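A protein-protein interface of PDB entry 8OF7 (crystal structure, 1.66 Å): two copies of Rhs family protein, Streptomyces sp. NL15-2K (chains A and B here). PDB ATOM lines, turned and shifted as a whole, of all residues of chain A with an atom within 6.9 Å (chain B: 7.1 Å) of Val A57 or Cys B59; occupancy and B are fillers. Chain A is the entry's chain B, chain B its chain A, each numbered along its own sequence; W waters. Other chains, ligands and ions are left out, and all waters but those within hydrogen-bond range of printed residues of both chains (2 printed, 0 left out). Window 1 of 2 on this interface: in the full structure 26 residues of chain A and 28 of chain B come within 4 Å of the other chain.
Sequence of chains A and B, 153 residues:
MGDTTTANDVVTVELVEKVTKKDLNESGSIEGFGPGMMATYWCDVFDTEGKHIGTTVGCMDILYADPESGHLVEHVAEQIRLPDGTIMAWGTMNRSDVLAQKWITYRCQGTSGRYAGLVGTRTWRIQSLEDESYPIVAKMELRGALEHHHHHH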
ATOM      1  N   GLU A  17       7.311 -41.403 -20.761  1.00  0.00           N
ATOM      2  CA  GLU A  17       7.533 -39.976 -20.537  1.00  0.00           C
ATOM      3  C   GLU A  17       8.986 -39.620 -20.836  1.00  0.00           C
ATOM      4  O   GLU A  17       9.892 -40.322 -20.377  1.00  0.00           O
ATOM      5  CB  GLU A  17       7.176 -39.616 -19.083  1.00  0.00           C
ATOM      6  CG  GLU A  17       5.734 -39.982 -18.776  1.00  0.00           C
ATOM      7  CD  GLU A  17       5.136 -39.539 -17.450  1.00  0.00           C
ATOM      8  OE1 GLU A  17       5.571 -38.486 -16.886  1.00  0.00           O
ATOM      9  OE2 GLU A  17       4.250 -40.287 -16.949  1.00  0.00           O
ATOM     10  N   THR A  40      12.933 -27.875 -11.469  1.00  0.00           N
ATOM     11  CA  THR A  40      11.625 -27.992 -12.103  1.00  0.00           C
ATOM     12  C   THR A  40      11.810 -28.655 -13.445  1.00  0.00           C
ATOM     13  O   THR A  40      12.886 -28.539 -14.033  1.00  0.00           O
ATOM     14  CB  THR A  40      10.935 -26.633 -12.298  1.00  0.00           C
ATOM     15  OG1 THR A  40      11.661 -25.639 -13.018  1.00  0.00           O
ATOM     16  CG2 THR A  40      10.513 -26.046 -10.968  1.00  0.00           C
ATOM     17  N   TYR A  41      10.749 -29.296 -13.920  1.00  0.00           N
ATOM     18  CA  TYR A  41      10.864 -30.030 -15.161  1.00  0.00           C
ATOM     19  C   TYR A  41       9.528 -30.196 -15.845  1.00  0.00           C
ATOM     20  O   TYR A  41       8.463 -30.106 -15.248  1.00  0.00           O
ATOM     21  CB  TYR A  41      11.593 -31.363 -14.920  1.00  0.00           C
ATOM     22  CG  TYR A  41      10.892 -32.291 -13.987  1.00  0.00           C
ATOM     23  CD1 TYR A  41       9.896 -33.135 -14.430  1.00  0.00           C
ATOM     24  CD2 TYR A  41      11.177 -32.290 -12.638  1.00  0.00           C
ATOM     25  CE1 TYR A  41       9.225 -33.982 -13.563  1.00  0.00           C
ATOM     26  CE2 TYR A  41      10.511 -33.133 -11.760  1.00  0.00           C
ATOM     27  CZ  TYR A  41       9.516 -33.968 -12.216  1.00  0.00           C
ATOM     28  OH  TYR A  41       8.829 -34.830 -11.359  1.00  0.00           O
ATOM     29  N   TRP A  42       9.642 -30.461 -17.139  1.00  0.00           N
ATOM     30  CA  TRP A  42       8.560 -30.755 -18.065  1.00  0.00           C
ATOM     31  C   TRP A  42       8.865 -32.065 -18.774  1.00  0.00           C
ATOM     32  O   TRP A  42      10.007 -32.225 -19.211  1.00  0.00           O
ATOM     33  CB  TRP A  42       8.449 -29.656 -19.123  1.00  0.00           C
ATOM     34  CG  TRP A  42       7.968 -28.336 -18.574  1.00  0.00           C
ATOM     35  CD1 TRP A  42       8.640 -27.487 -17.741  1.00  0.00           C
ATOM     36  CD2 TRP A  42       6.697 -27.736 -18.829  1.00  0.00           C
ATOM     37  NE1 TRP A  42       7.871 -26.388 -17.470  1.00  0.00           N
ATOM     38  CE2 TRP A  42       6.694 -26.504 -18.146  1.00  0.00           C
ATOM     39  CE3 TRP A  42       5.597 -28.097 -19.606  1.00  0.00           C
ATOM     40  CZ2 TRP A  42       5.570 -25.690 -18.135  1.00  0.00           C
ATOM     41  CZ3 TRP A  42       4.505 -27.262 -19.645  1.00  0.00           C
ATOM     42  CH2 TRP A  42       4.504 -26.084 -18.910  1.00  0.00           C
ATOM     43  N   CYS A  43       7.824 -32.866 -19.009  1.00  0.00           N
ATOM     44  CA  CYS A  43       7.932 -34.059 -19.843  1.00  0.00           C
ATOM     45  C   CYS A  43       6.766 -34.189 -20.820  1.00  0.00           C
ATOM     46  O   CYS A  43       5.622 -33.864 -20.506  1.00  0.00           O
ATOM     47  CB  CYS A  43       7.986 -35.333 -19.005  1.00  0.00           C
ATOM     48  SG  CYS A  43       9.230 -35.250 -17.697  1.00  0.00           S
ATOM     49  N   THR A  55       1.230 -34.244 -20.827  1.00  0.00           N
ATOM     50  CA  THR A  55       2.353 -33.492 -20.324  1.00  0.00           C
ATOM     51  C   THR A  55       2.464 -33.739 -18.828  1.00  0.00           C
ATOM     52  O   THR A  55       1.450 -33.719 -18.100  1.00  0.00           O
ATOM     53  CB  THR A  55       2.154 -31.986 -20.590  1.00  0.00           C
ATOM     54  OG1 THR A  55       1.937 -31.744 -21.969  1.00  0.00           O
ATOM     55  CG2 THR A  55       3.341 -31.128 -20.205  1.00  0.00           C
ATOM     56  N   THR A  56       3.702 -33.828 -18.351  1.00  0.00           N
ATOM     57  CA  THR A  56       3.985 -33.811 -16.910  1.00  0.00           C
ATOM     58  C   THR A  56       4.797 -32.561 -16.553  1.00  0.00           C
ATOM     59  O   THR A  56       5.727 -32.194 -17.260  1.00  0.00           O
ATOM     60  CB  THR A  56       4.761 -35.070 -16.492  1.00  0.00           C
ATOM     61  OG1 THR A  56       3.965 -36.226 -16.747  1.00  0.00           O
ATOM     62  CG2 THR A  56       5.230 -35.042 -15.054  1.00  0.00           C
ATOM     63  N   VAL A  57       4.439 -31.897 -15.435  1.00  0.00           N
ATOM     64  CA  VAL A  57       5.235 -30.832 -14.848  1.00  0.00           C
ATOM     65  C   VAL A  57       5.553 -31.259 -13.428  1.00  0.00           C
ATOM     66  O   VAL A  57       4.749 -31.937 -12.798  1.00  0.00           O
ATOM     67  CB  VAL A  57       4.553 -29.441 -14.876  1.00  0.00           C
ATOM     68  CG1 VAL A  57       4.472 -28.871 -16.288  1.00  0.00           C
ATOM     69  CG2 VAL A  57       3.155 -29.453 -14.275  1.00  0.00           C
ATOM     70  N   GLY A  58       6.746 -30.909 -12.940  1.00  0.00           N
ATOM     71  CA  GLY A  58       7.182 -31.383 -11.658  1.00  0.00           C
ATOM     72  C   GLY A  58       8.234 -30.491 -11.015  1.00  0.00           C
ATOM     73  O   GLY A  58       8.830 -29.600 -11.645  1.00  0.00           O
ATOM     74  N   CYS A  59       8.426 -30.755  -9.723  1.00  0.00           N
ATOM     75  CA  CYS A  59       9.458 -30.095  -8.988  1.00  0.00           C
ATOM     76  C   CYS A  59      10.109 -31.108  -8.037  1.00  0.00           C
ATOM     77  O   CYS A  59       9.524 -32.159  -7.683  1.00  0.00           O
ATOM     78  CB  CYS A  59       8.900 -28.870  -8.280  1.00  0.00           C
ATOM     79  SG  CYS A  59       7.674 -29.280  -7.019  1.00  0.00           S
ATOM     80  N   ALA A  77       7.237 -33.702  -6.423  1.00  0.00           N
ATOM     81  CA  ALA A  77       5.799 -33.486  -6.547  1.00  0.00           C
ATOM     82  C   ALA A  77       5.517 -33.094  -7.995  1.00  0.00           C
ATOM     83  O   ALA A  77       6.209 -32.237  -8.542  1.00  0.00           O
ATOM     84  CB  ALA A  77       5.401 -32.430  -5.554  1.00  0.00           C
ATOM     85  N   GLU A  78       4.566 -33.748  -8.643  1.00  0.00           N
ATOM     86  CA  GLU A  78       4.351 -33.536 -10.054  1.00  0.00           C
ATOM     87  C   GLU A  78       2.877 -33.670 -10.391  1.00  0.00           C
ATOM     88  O   GLU A  78       2.095 -34.179  -9.598  1.00  0.00           O
ATOM     89  CB  GLU A  78       5.252 -34.460 -10.865  1.00  0.00           C
ATOM     90  CG  GLU A  78       4.969 -35.892 -10.620  1.00  0.00           C
ATOM     91  CD  GLU A  78       5.934 -36.870 -11.319  1.00  0.00           C
ATOM     92  OE1 GLU A  78       6.926 -36.446 -11.972  1.00  0.00           O
ATOM     93  OE2 GLU A  78       5.665 -38.064 -11.212  1.00  0.00           O
ATOM     94  N   GLN A  79       2.544 -33.180 -11.567  1.00  0.00           N
ATOM     95  CA  GLN A  79       1.196 -33.226 -12.085  1.00  0.00           C
ATOM     96  C   GLN A  79       1.263 -33.724 -13.506  1.00  0.00           C
ATOM     97  O   GLN A  79       2.091 -33.239 -14.268  1.00  0.00           O
ATOM     98  CB  GLN A  79       0.508 -31.872 -11.956  1.00  0.00           C
ATOM     99  CG  GLN A  79       0.539 -31.402 -10.499  1.00  0.00           C
ATOM    100  CD  GLN A  79      -0.421 -30.255 -10.273  1.00  0.00           C
ATOM    101  OE1 GLN A  79      -1.613 -30.452 -10.107  1.00  0.00           O
ATOM    102  NE2 GLN A  79       0.089 -29.043 -10.271  1.00  0.00           N
ATOM    103  N   ILE A  80       0.316 -34.612 -13.811  1.00  0.00           N
ATOM    104  CA  ILE A  80       0.260 -35.234 -15.111  1.00  0.00           C
ATOM    105  C   ILE A  80      -1.081 -34.906 -15.714  1.00  0.00           C
ATOM    106  O   ILE A  80      -2.102 -35.149 -15.067  1.00  0.00           O
ATOM    107  CB  ILE A  80       0.466 -36.755 -14.980  1.00  0.00           C
ATOM    108  CG1 ILE A  80       1.744 -37.102 -14.221  1.00  0.00           C
ATOM    109  CG2 ILE A  80       0.438 -37.397 -16.368  1.00  0.00           C
ATOM    110  CD1 ILE A  80       1.554 -37.542 -12.784  1.00  0.00           C
ATOM    111  N   ARG A  81      -1.051 -34.397 -16.947  1.00  0.00           N
ATOM    112  CA  ARG A  81      -2.254 -34.078 -17.688  1.00  0.00           C
ATOM    113  C   ARG A  81      -2.413 -35.079 -18.822  1.00  0.00           C
ATOM    114  O   ARG A  81      -1.462 -35.272 -19.574  1.00  0.00           O
ATOM    115  CB  ARG A  81      -2.163 -32.657 -18.258  1.00  0.00           C
ATOM    116  CG  ARG A  81      -3.258 -32.304 -19.255  1.00  0.00           C
ATOM    117  CD  ARG A  81      -3.285 -30.812 -19.598  1.00  0.00           C
ATOM    118  NE  ARG A  81      -4.666 -30.392 -19.444  1.00  0.00           N
ATOM    119  CZ  ARG A  81      -5.135 -29.765 -18.384  1.00  0.00           C
ATOM    120  NH1 ARG A  81      -6.414 -29.885 -18.067  1.00  0.00           N
ATOM    121  NH2 ARG A  81      -4.306 -29.116 -17.583  1.00  0.00           N
ATOM    122  N   ASP B  23       7.606 -20.643 -16.327  1.00  0.00           N
ATOM    123  CA  ASP B  23       7.489 -21.172 -17.672  1.00  0.00           C
ATOM    124  C   ASP B  23       6.098 -21.722 -17.849  1.00  0.00           C
ATOM    125  O   ASP B  23       5.620 -22.428 -16.963  1.00  0.00           O
ATOM    126  CB  ASP B  23       8.536 -22.263 -17.897  1.00  0.00           C
ATOM    127  CG  ASP B  23       9.986 -21.756 -17.912  1.00  0.00           C
ATOM    128  OD1 ASP B  23      10.488 -21.428 -19.012  1.00  0.00           O
ATOM    129  OD2 ASP B  23      10.622 -21.789 -16.843  1.00  0.00           O
ATOM    130  N   ASN B  25       3.146 -23.710 -20.804  1.00  0.00           N
ATOM    131  CA  ASN B  25       3.143 -24.609 -21.960  1.00  0.00           C
ATOM    132  C   ASN B  25       3.187 -23.784 -23.245  1.00  0.00           C
ATOM    133  O   ASN B  25       2.499 -22.785 -23.381  1.00  0.00           O
ATOM    134  CB  ASN B  25       1.949 -25.582 -21.978  1.00  0.00           C
ATOM    135  CG  ASN B  25       0.603 -24.867 -22.071  1.00  0.00           C
ATOM    136  OD1 ASN B  25      -0.123 -24.854 -23.075  1.00  0.00           O
ATOM    137  ND2 ASN B  25       0.320 -24.172 -21.011  1.00  0.00           N
ATOM    138  N   MET B  38      -0.594 -25.099 -18.076  1.00  0.00           N
ATOM    139  CA  MET B  38       0.340 -25.657 -17.094  1.00  0.00           C
ATOM    140  C   MET B  38       1.514 -24.710 -16.945  1.00  0.00           C
ATOM    141  O   MET B  38       1.835 -23.962 -17.872  1.00  0.00           O
ATOM    142  CB  MET B  38       0.897 -27.002 -17.599  1.00  0.00           C
ATOM    143  CG  MET B  38      -0.192 -28.006 -17.772  1.00  0.00           C
ATOM    144  SD  MET B  38       0.329 -29.602 -18.467  1.00  0.00           S
ATOM    145  CE  MET B  38       0.778 -30.393 -16.927  1.00  0.00           C
ATOM    146  N   ALA B  39       2.191 -24.767 -15.803  1.00  0.00           N
ATOM    147  CA  ALA B  39       3.331 -23.911 -15.535  1.00  0.00           C
ATOM    148  C   ALA B  39       4.273 -24.592 -14.554  1.00  0.00           C
ATOM    149  O   ALA B  39       3.831 -25.393 -13.720  1.00  0.00           O
ATOM    150  CB  ALA B  39       2.905 -22.578 -14.930  1.00  0.00           C
ATOM    151  N   THR B  40       5.558 -24.216 -14.620  1.00  0.00           N
ATOM    152  CA  THR B  40       6.464 -24.380 -13.479  1.00  0.00           C
ATOM    153  C   THR B  40       6.974 -23.019 -13.043  1.00  0.00           C
ATOM    154  O   THR B  40       7.115 -22.111 -13.860  1.00  0.00           O
ATOM    155  CB  THR B  40       7.650 -25.279 -13.856  1.00  0.00           C
ATOM    156  OG1 THR B  40       8.307 -24.797 -15.023  1.00  0.00           O
ATOM    157  CG2 THR B  40       7.196 -26.702 -14.085  1.00  0.00           C
ATOM    158  N   TYR B  41       7.368 -22.871 -11.772  1.00  0.00           N
ATOM    159  CA  TYR B  41       7.861 -21.601 -11.304  1.00  0.00           C
ATOM    160  C   TYR B  41       8.838 -21.805 -10.171  1.00  0.00           C
ATOM    161  O   TYR B  41       8.812 -22.854  -9.522  1.00  0.00           O
ATOM    162  CB  TYR B  41       6.719 -20.691 -10.791  1.00  0.00           C
ATOM    163  CG  TYR B  41       5.825 -21.321  -9.767  1.00  0.00           C
ATOM    164  CD1 TYR B  41       4.720 -22.076 -10.102  1.00  0.00           C
ATOM    165  CD2 TYR B  41       6.098 -21.150  -8.421  1.00  0.00           C
ATOM    166  CE1 TYR B  41       3.931 -22.674  -9.120  1.00  0.00           C
ATOM    167  CE2 TYR B  41       5.304 -21.705  -7.430  1.00  0.00           C
ATOM    168  CZ  TYR B  41       4.214 -22.493  -7.783  1.00  0.00           C
ATOM    169  OH  TYR B  41       3.424 -23.092  -6.791  1.00  0.00           O
ATOM    170  N   VAL B  57       9.787 -24.034  -5.267  1.00  0.00           N
ATOM    171  CA  VAL B  57       9.635 -24.479  -6.636  1.00  0.00           C
ATOM    172  C   VAL B  57       8.244 -25.089  -6.741  1.00  0.00           C
ATOM    173  O   VAL B  57       7.778 -25.748  -5.811  1.00  0.00           O
ATOM    174  CB  VAL B  57      10.690 -25.529  -7.049  1.00  0.00           C
ATOM    175  CG1 VAL B  57      12.065 -24.902  -7.366  1.00  0.00           C
ATOM    176  CG2 VAL B  57      10.793 -26.672  -6.040  1.00  0.00           C
ATOM    177  N   GLY B  58       7.562 -24.916  -7.876  1.00  0.00           N
ATOM    178  CA  GLY B  58       6.202 -25.408  -7.976  1.00  0.00           C
ATOM    179  C   GLY B  58       5.732 -25.669  -9.383  1.00  0.00           C
ATOM    180  O   GLY B  58       6.400 -25.282 -10.355  1.00  0.00           O
ATOM    181  N   CYS B  59       4.564 -26.319  -9.470  1.00  0.00           N
ATOM    182  CA  CYS B  59       3.954 -26.595 -10.753  1.00  0.00           C
ATOM    183  C   CYS B  59       2.438 -26.406 -10.633  1.00  0.00           C
ATOM    184  O   CYS B  59       1.864 -26.475  -9.541  1.00  0.00           O
ATOM    185  CB  CYS B  59       4.424 -27.953 -11.261  1.00  0.00           C
ATOM    186  SG  CYS B  59       3.779 -29.306 -10.277  1.00  0.00           S
ATOM    187  N   MET B  60       1.832 -26.077 -11.760  1.00  0.00           N
ATOM    188  CA  MET B  60       0.417 -25.720 -11.810  1.00  0.00           C
ATOM    189  C   MET B  60      -0.177 -26.424 -12.991  1.00  0.00           C
ATOM    190  O   MET B  60       0.459 -26.535 -14.025  1.00  0.00           O
ATOM    191  CB  MET B  60       0.296 -24.191 -11.945  1.00  0.00           C
ATOM    192  CG  MET B  60      -1.113 -23.643 -12.139  1.00  0.00           C
ATOM    193  SD  MET B  60      -1.879 -23.877 -13.756  1.00  0.00           S
ATOM    194  CE  MET B  60      -1.070 -22.602 -14.718  1.00  0.00           C
ATOM    195  N   ASP B  61      -1.447 -26.832 -12.855  1.00  0.00           N
ATOM    196  CA  ASP B  61      -2.226 -27.404 -13.926  1.00  0.00           C
ATOM    197  C   ASP B  61      -3.644 -26.810 -13.825  1.00  0.00           C
ATOM    198  O   ASP B  61      -4.207 -26.734 -12.728  1.00  0.00           O
ATOM    199  CB  ASP B  61      -2.254 -28.904 -13.661  1.00  0.00           C
ATOM    200  CG  ASP B  61      -2.536 -29.844 -14.802  1.00  0.00           C
ATOM    201  OD1 ASP B  61      -2.622 -29.358 -15.925  1.00  0.00           O
ATOM    202  OD2 ASP B  61      -2.687 -31.080 -14.514  1.00  0.00           O
ATOM    203  N   HIS B  75      -4.784 -26.333 -10.031  1.00  0.00           N
ATOM    204  CA  HIS B  75      -4.218 -27.140  -8.973  1.00  0.00           C
ATOM    205  C   HIS B  75      -2.695 -26.955  -8.961  1.00  0.00           C
ATOM    206  O   HIS B  75      -2.068 -26.967  -9.992  1.00  0.00           O
ATOM    207  CB  HIS B  75      -4.549 -28.617  -9.207  1.00  0.00           C
ATOM    208  CG  HIS B  75      -4.314 -29.457  -7.994  1.00  0.00           C
ATOM    209  ND1 HIS B  75      -3.121 -30.105  -7.732  1.00  0.00           N
ATOM    210  CD2 HIS B  75      -5.102 -29.665  -6.914  1.00  0.00           C
ATOM    211  CE1 HIS B  75      -3.238 -30.739  -6.557  1.00  0.00           C
ATOM    212  NE2 HIS B  75      -4.434 -30.465  -6.038  1.00  0.00           N
ATOM    213  N   VAL B  76      -2.142 -26.816  -7.777  1.00  0.00           N
ATOM    214  CA  VAL B  76      -0.746 -26.513  -7.527  1.00  0.00           C
ATOM    215  C   VAL B  76      -0.133 -27.583  -6.616  1.00  0.00           C
ATOM    216  O   VAL B  76      -0.740 -28.102  -5.670  1.00  0.00           O
ATOM    217  CB  VAL B  76      -0.573 -25.104  -6.905  1.00  0.00           C
ATOM    218  CG1 VAL B  76       0.787 -24.838  -6.276  1.00  0.00           C
ATOM    219  CG2 VAL B  76      -0.847 -24.035  -7.957  1.00  0.00           C
ATOM    220  N   ALA B  77       1.115 -27.956  -6.941  1.00  0.00           N
ATOM    221  CA  ALA B  77       1.938 -28.739  -6.039  1.00  0.00           C
ATOM    222  C   ALA B  77       3.292 -28.039  -5.965  1.00  0.00           C
ATOM    223  O   ALA B  77       3.821 -27.558  -6.960  1.00  0.00           O
ATOM    224  CB  ALA B  77       2.054 -30.168  -6.517  1.00  0.00           C
ATOM    225  N   GLU B  78       3.799 -27.801  -4.771  1.00  0.00           N
ATOM    226  CA  GLU B  78       5.020 -27.049  -4.645  1.00  0.00           C
ATOM    227  C   GLU B  78       5.843 -27.525  -3.442  1.00  0.00           C
ATOM    228  O   GLU B  78       5.361 -28.205  -2.537  1.00  0.00           O
ATOM    229  CB  GLU B  78       4.698 -25.563  -4.553  1.00  0.00           C
ATOM    230  CG  GLU B  78       3.960 -25.184  -3.332  1.00  0.00           C
ATOM    231  CD  GLU B  78       3.476 -23.741  -3.349  1.00  0.00           C
ATOM    232  OE1 GLU B  78       3.735 -23.001  -4.347  1.00  0.00           O
ATOM    233  OE2 GLU B  78       2.788 -23.385  -2.368  1.00  0.00           O
ATOM    234  N   GLN B  79       7.107 -27.149  -3.456  1.00  0.00           N
ATOM    235  CA  GLN B  79       7.984 -27.458  -2.332  1.00  0.00           C
ATOM    236  C   GLN B  79       8.777 -26.239  -1.915  1.00  0.00           C
ATOM    237  O   GLN B  79       9.240 -25.464  -2.729  1.00  0.00           O
ATOM    238  CB  GLN B  79       8.964 -28.564  -2.767  1.00  0.00           C
ATOM    239  CG  GLN B  79       8.226 -29.847  -3.123  1.00  0.00           C
ATOM    240  CD  GLN B  79       9.114 -31.060  -3.219  1.00  0.00           C
ATOM    241  OE1 GLN B  79       9.418 -31.686  -2.226  1.00  0.00           O
ATOM    242  NE2 GLN B  79       9.499 -31.423  -4.425  1.00  0.00           N
ATOM    243  N   TYR B 106      -4.034 -23.946   1.234  1.00  0.00           N
ATOM    244  CA  TYR B 106      -3.468 -25.192   0.748  1.00  0.00           C
ATOM    245  C   TYR B 106      -3.156 -26.115   1.937  1.00  0.00           C
ATOM    246  O   TYR B 106      -2.917 -25.660   3.045  1.00  0.00           O
ATOM    247  CB  TYR B 106      -2.093 -24.975   0.092  1.00  0.00           C
ATOM    248  CG  TYR B 106      -2.010 -24.375  -1.286  1.00  0.00           C
ATOM    249  CD1 TYR B 106      -3.127 -24.042  -2.009  1.00  0.00           C
ATOM    250  CD2 TYR B 106      -0.767 -24.060  -1.842  1.00  0.00           C
ATOM    251  CE1 TYR B 106      -3.042 -23.468  -3.271  1.00  0.00           C
ATOM    252  CE2 TYR B 106      -0.664 -23.427  -3.078  1.00  0.00           C
ATOM    253  CZ  TYR B 106      -1.817 -23.126  -3.799  1.00  0.00           C
ATOM    254  OH  TYR B 106      -1.841 -22.580  -5.085  1.00  0.00           O
HETATM  255  O   HOH W   1      11.133 -26.074 -15.579  1.00  0.00           O
HETATM  256  O   HOH W   2      10.240 -22.860 -14.553  1.00  0.00           O
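Of the 15 printed residues of chain A, 9 touch a printed residue of chain B. Hydrophobic or aromatic side chains of chain A within 4 Å of the printed part of chain B: Trp A42 and Val A57. Hydrophobic or aromatic side chains of chain B that line the printed part of chain A: Met B38, Val B57 and His B75. Along chain B the printed residues that touch a printed residue of chain A span positions 23 to 79. Among the printed residues, Asp or Glu carboxylates within 4 Å of a Lys or Arg side-chain nitrogen of the other chain: Arg A81 with Asp B61.
The backbone NH of Asp B23 is in hydrogen-bond range of the backbone carbonyl oxygen of Thr B40 (2.9 Å). N of Met B38 sits close to ND2 of Asn B25 (3.2 Å). O of Val B57 is in hydrogen-bond range of N of Gln B79 (2.8 Å). The backbone NH of His B75 sits at hydrogen-bond distance from the backbone carbonyl oxygen of Asp B61. The backbone NH of Gly A58 is in hydrogen-bond range of the backbone carbonyl oxygen of Tyr A41 (3.0 Å). The backbone carbonyl oxygen (O) of Ala A77 lies within hydrogen-bond range of the backbone NH (N) of Cys A59 (2.9 Å).
OG1 of Thr B40 sits at hydrogen-bond distance from NE1 of Trp A42, at 3.0 Å. The side-chain sulfur (SG) of Cys A59 is in hydrogen-bond range of the backbone carbonyl oxygen (O) of Val B57 (3.7 Å). The side-chain sulfur (SG) of Cys B59 sits at hydrogen-bond distance from the backbone carbonyl oxygen (O) of Val A57 (3.8 Å). O of Cys B59 is in hydrogen-bond range of NE2 of Gln A79, at 3.2 Å. The side-chain carboxylate (OD2) of Asp B61 is in salt-bridge range of the guanidinium group (NH2) of Arg A81, at 3.99 Å. ND1 of His B75 is in hydrogen-bond range of OE1 of Gln A79. The side-chain amide nitrogen (NE2) of Gln B79 is in hydrogen-bond range of the backbone carbonyl oxygen (O) of Cys A59 (3.3 Å).
Thr B40 touches its own counterpart, Thr A40. Val A57 touches Cys B59, and with the chains exchanged Cys A59 touches Val B57. Cys A59 touches Gln B79, and with the chains exchanged Gln A79 touches Cys B59. Ala A77 touches Gln B79, and with the chains exchanged Gln A79 touches Ala B77. 8 positions are printed for both chains. Of the 25 pairs that touch across the chains among the printed residues, 11 have their exchanged pair printed and touching as well.
Water W2 lies within hydrogen-bond range of OD2 of Asp B23 (2.6 Å), OG1 of Thr B40 (2.8 Å) and OG1 of Thr A40 (3.5 Å). Water W1 lies within hydrogen-bond range of the side-chain hydroxyl (OG1) of Thr A40 (2.7 Å) and the side-chain hydroxyl (OG1) of Thr B40 (3.2 Å).
Among the printed residues, merely in contact across the chains: Trp A42 with Asn B25 (3.3 Å), Trp A42 with Asp B23 (3.5 Å), Trp A42 with Met B38 (3.6 Å), Thr A55 with Met B38 (3.6 Å), Gln A79 with Ala B77 (3.7 Å), Gln A79 with Met B60 (3.7 Å), Val A57 with Met B38 (3.7 Å), Gln A79 with Asp B61 (3.7 Å), Ala A77 with Gln B79 (3.8 Å), Tyr A41 with Thr B40 (3.8 Å), Gln A79 with Val B76 (3.8 Å), Trp A42 with Ala B39 (3.9 Å), Thr A40 with Thr B40 (3.9 Å), Val A57 with Thr B40 (3.9 Å), Thr A40 with Tyr B41 (3.9 Å), Arg A81 with Met B38 (3.9 Å), Thr A40 with Val B57 (3.96 Å) and Val A57 with Met B60 (3.98 Å).
Cys B59 touches two residues of chain A. Of the printed residues of chain A, Ala B77 touches Gln A79. Printed residues of chain A within 4 Å of Thr B40: Thr A40, Tyr A41, Trp A42 and Val A57. Glu A17 touches none of the printed residues of chain B. The nearest printed residue of chain B that does not touch Val A57 is Ala B39 (4.2 Å). The nearest printed residue of chain A that does not touch Tyr B41 is Cys A59 (6.1 Å).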
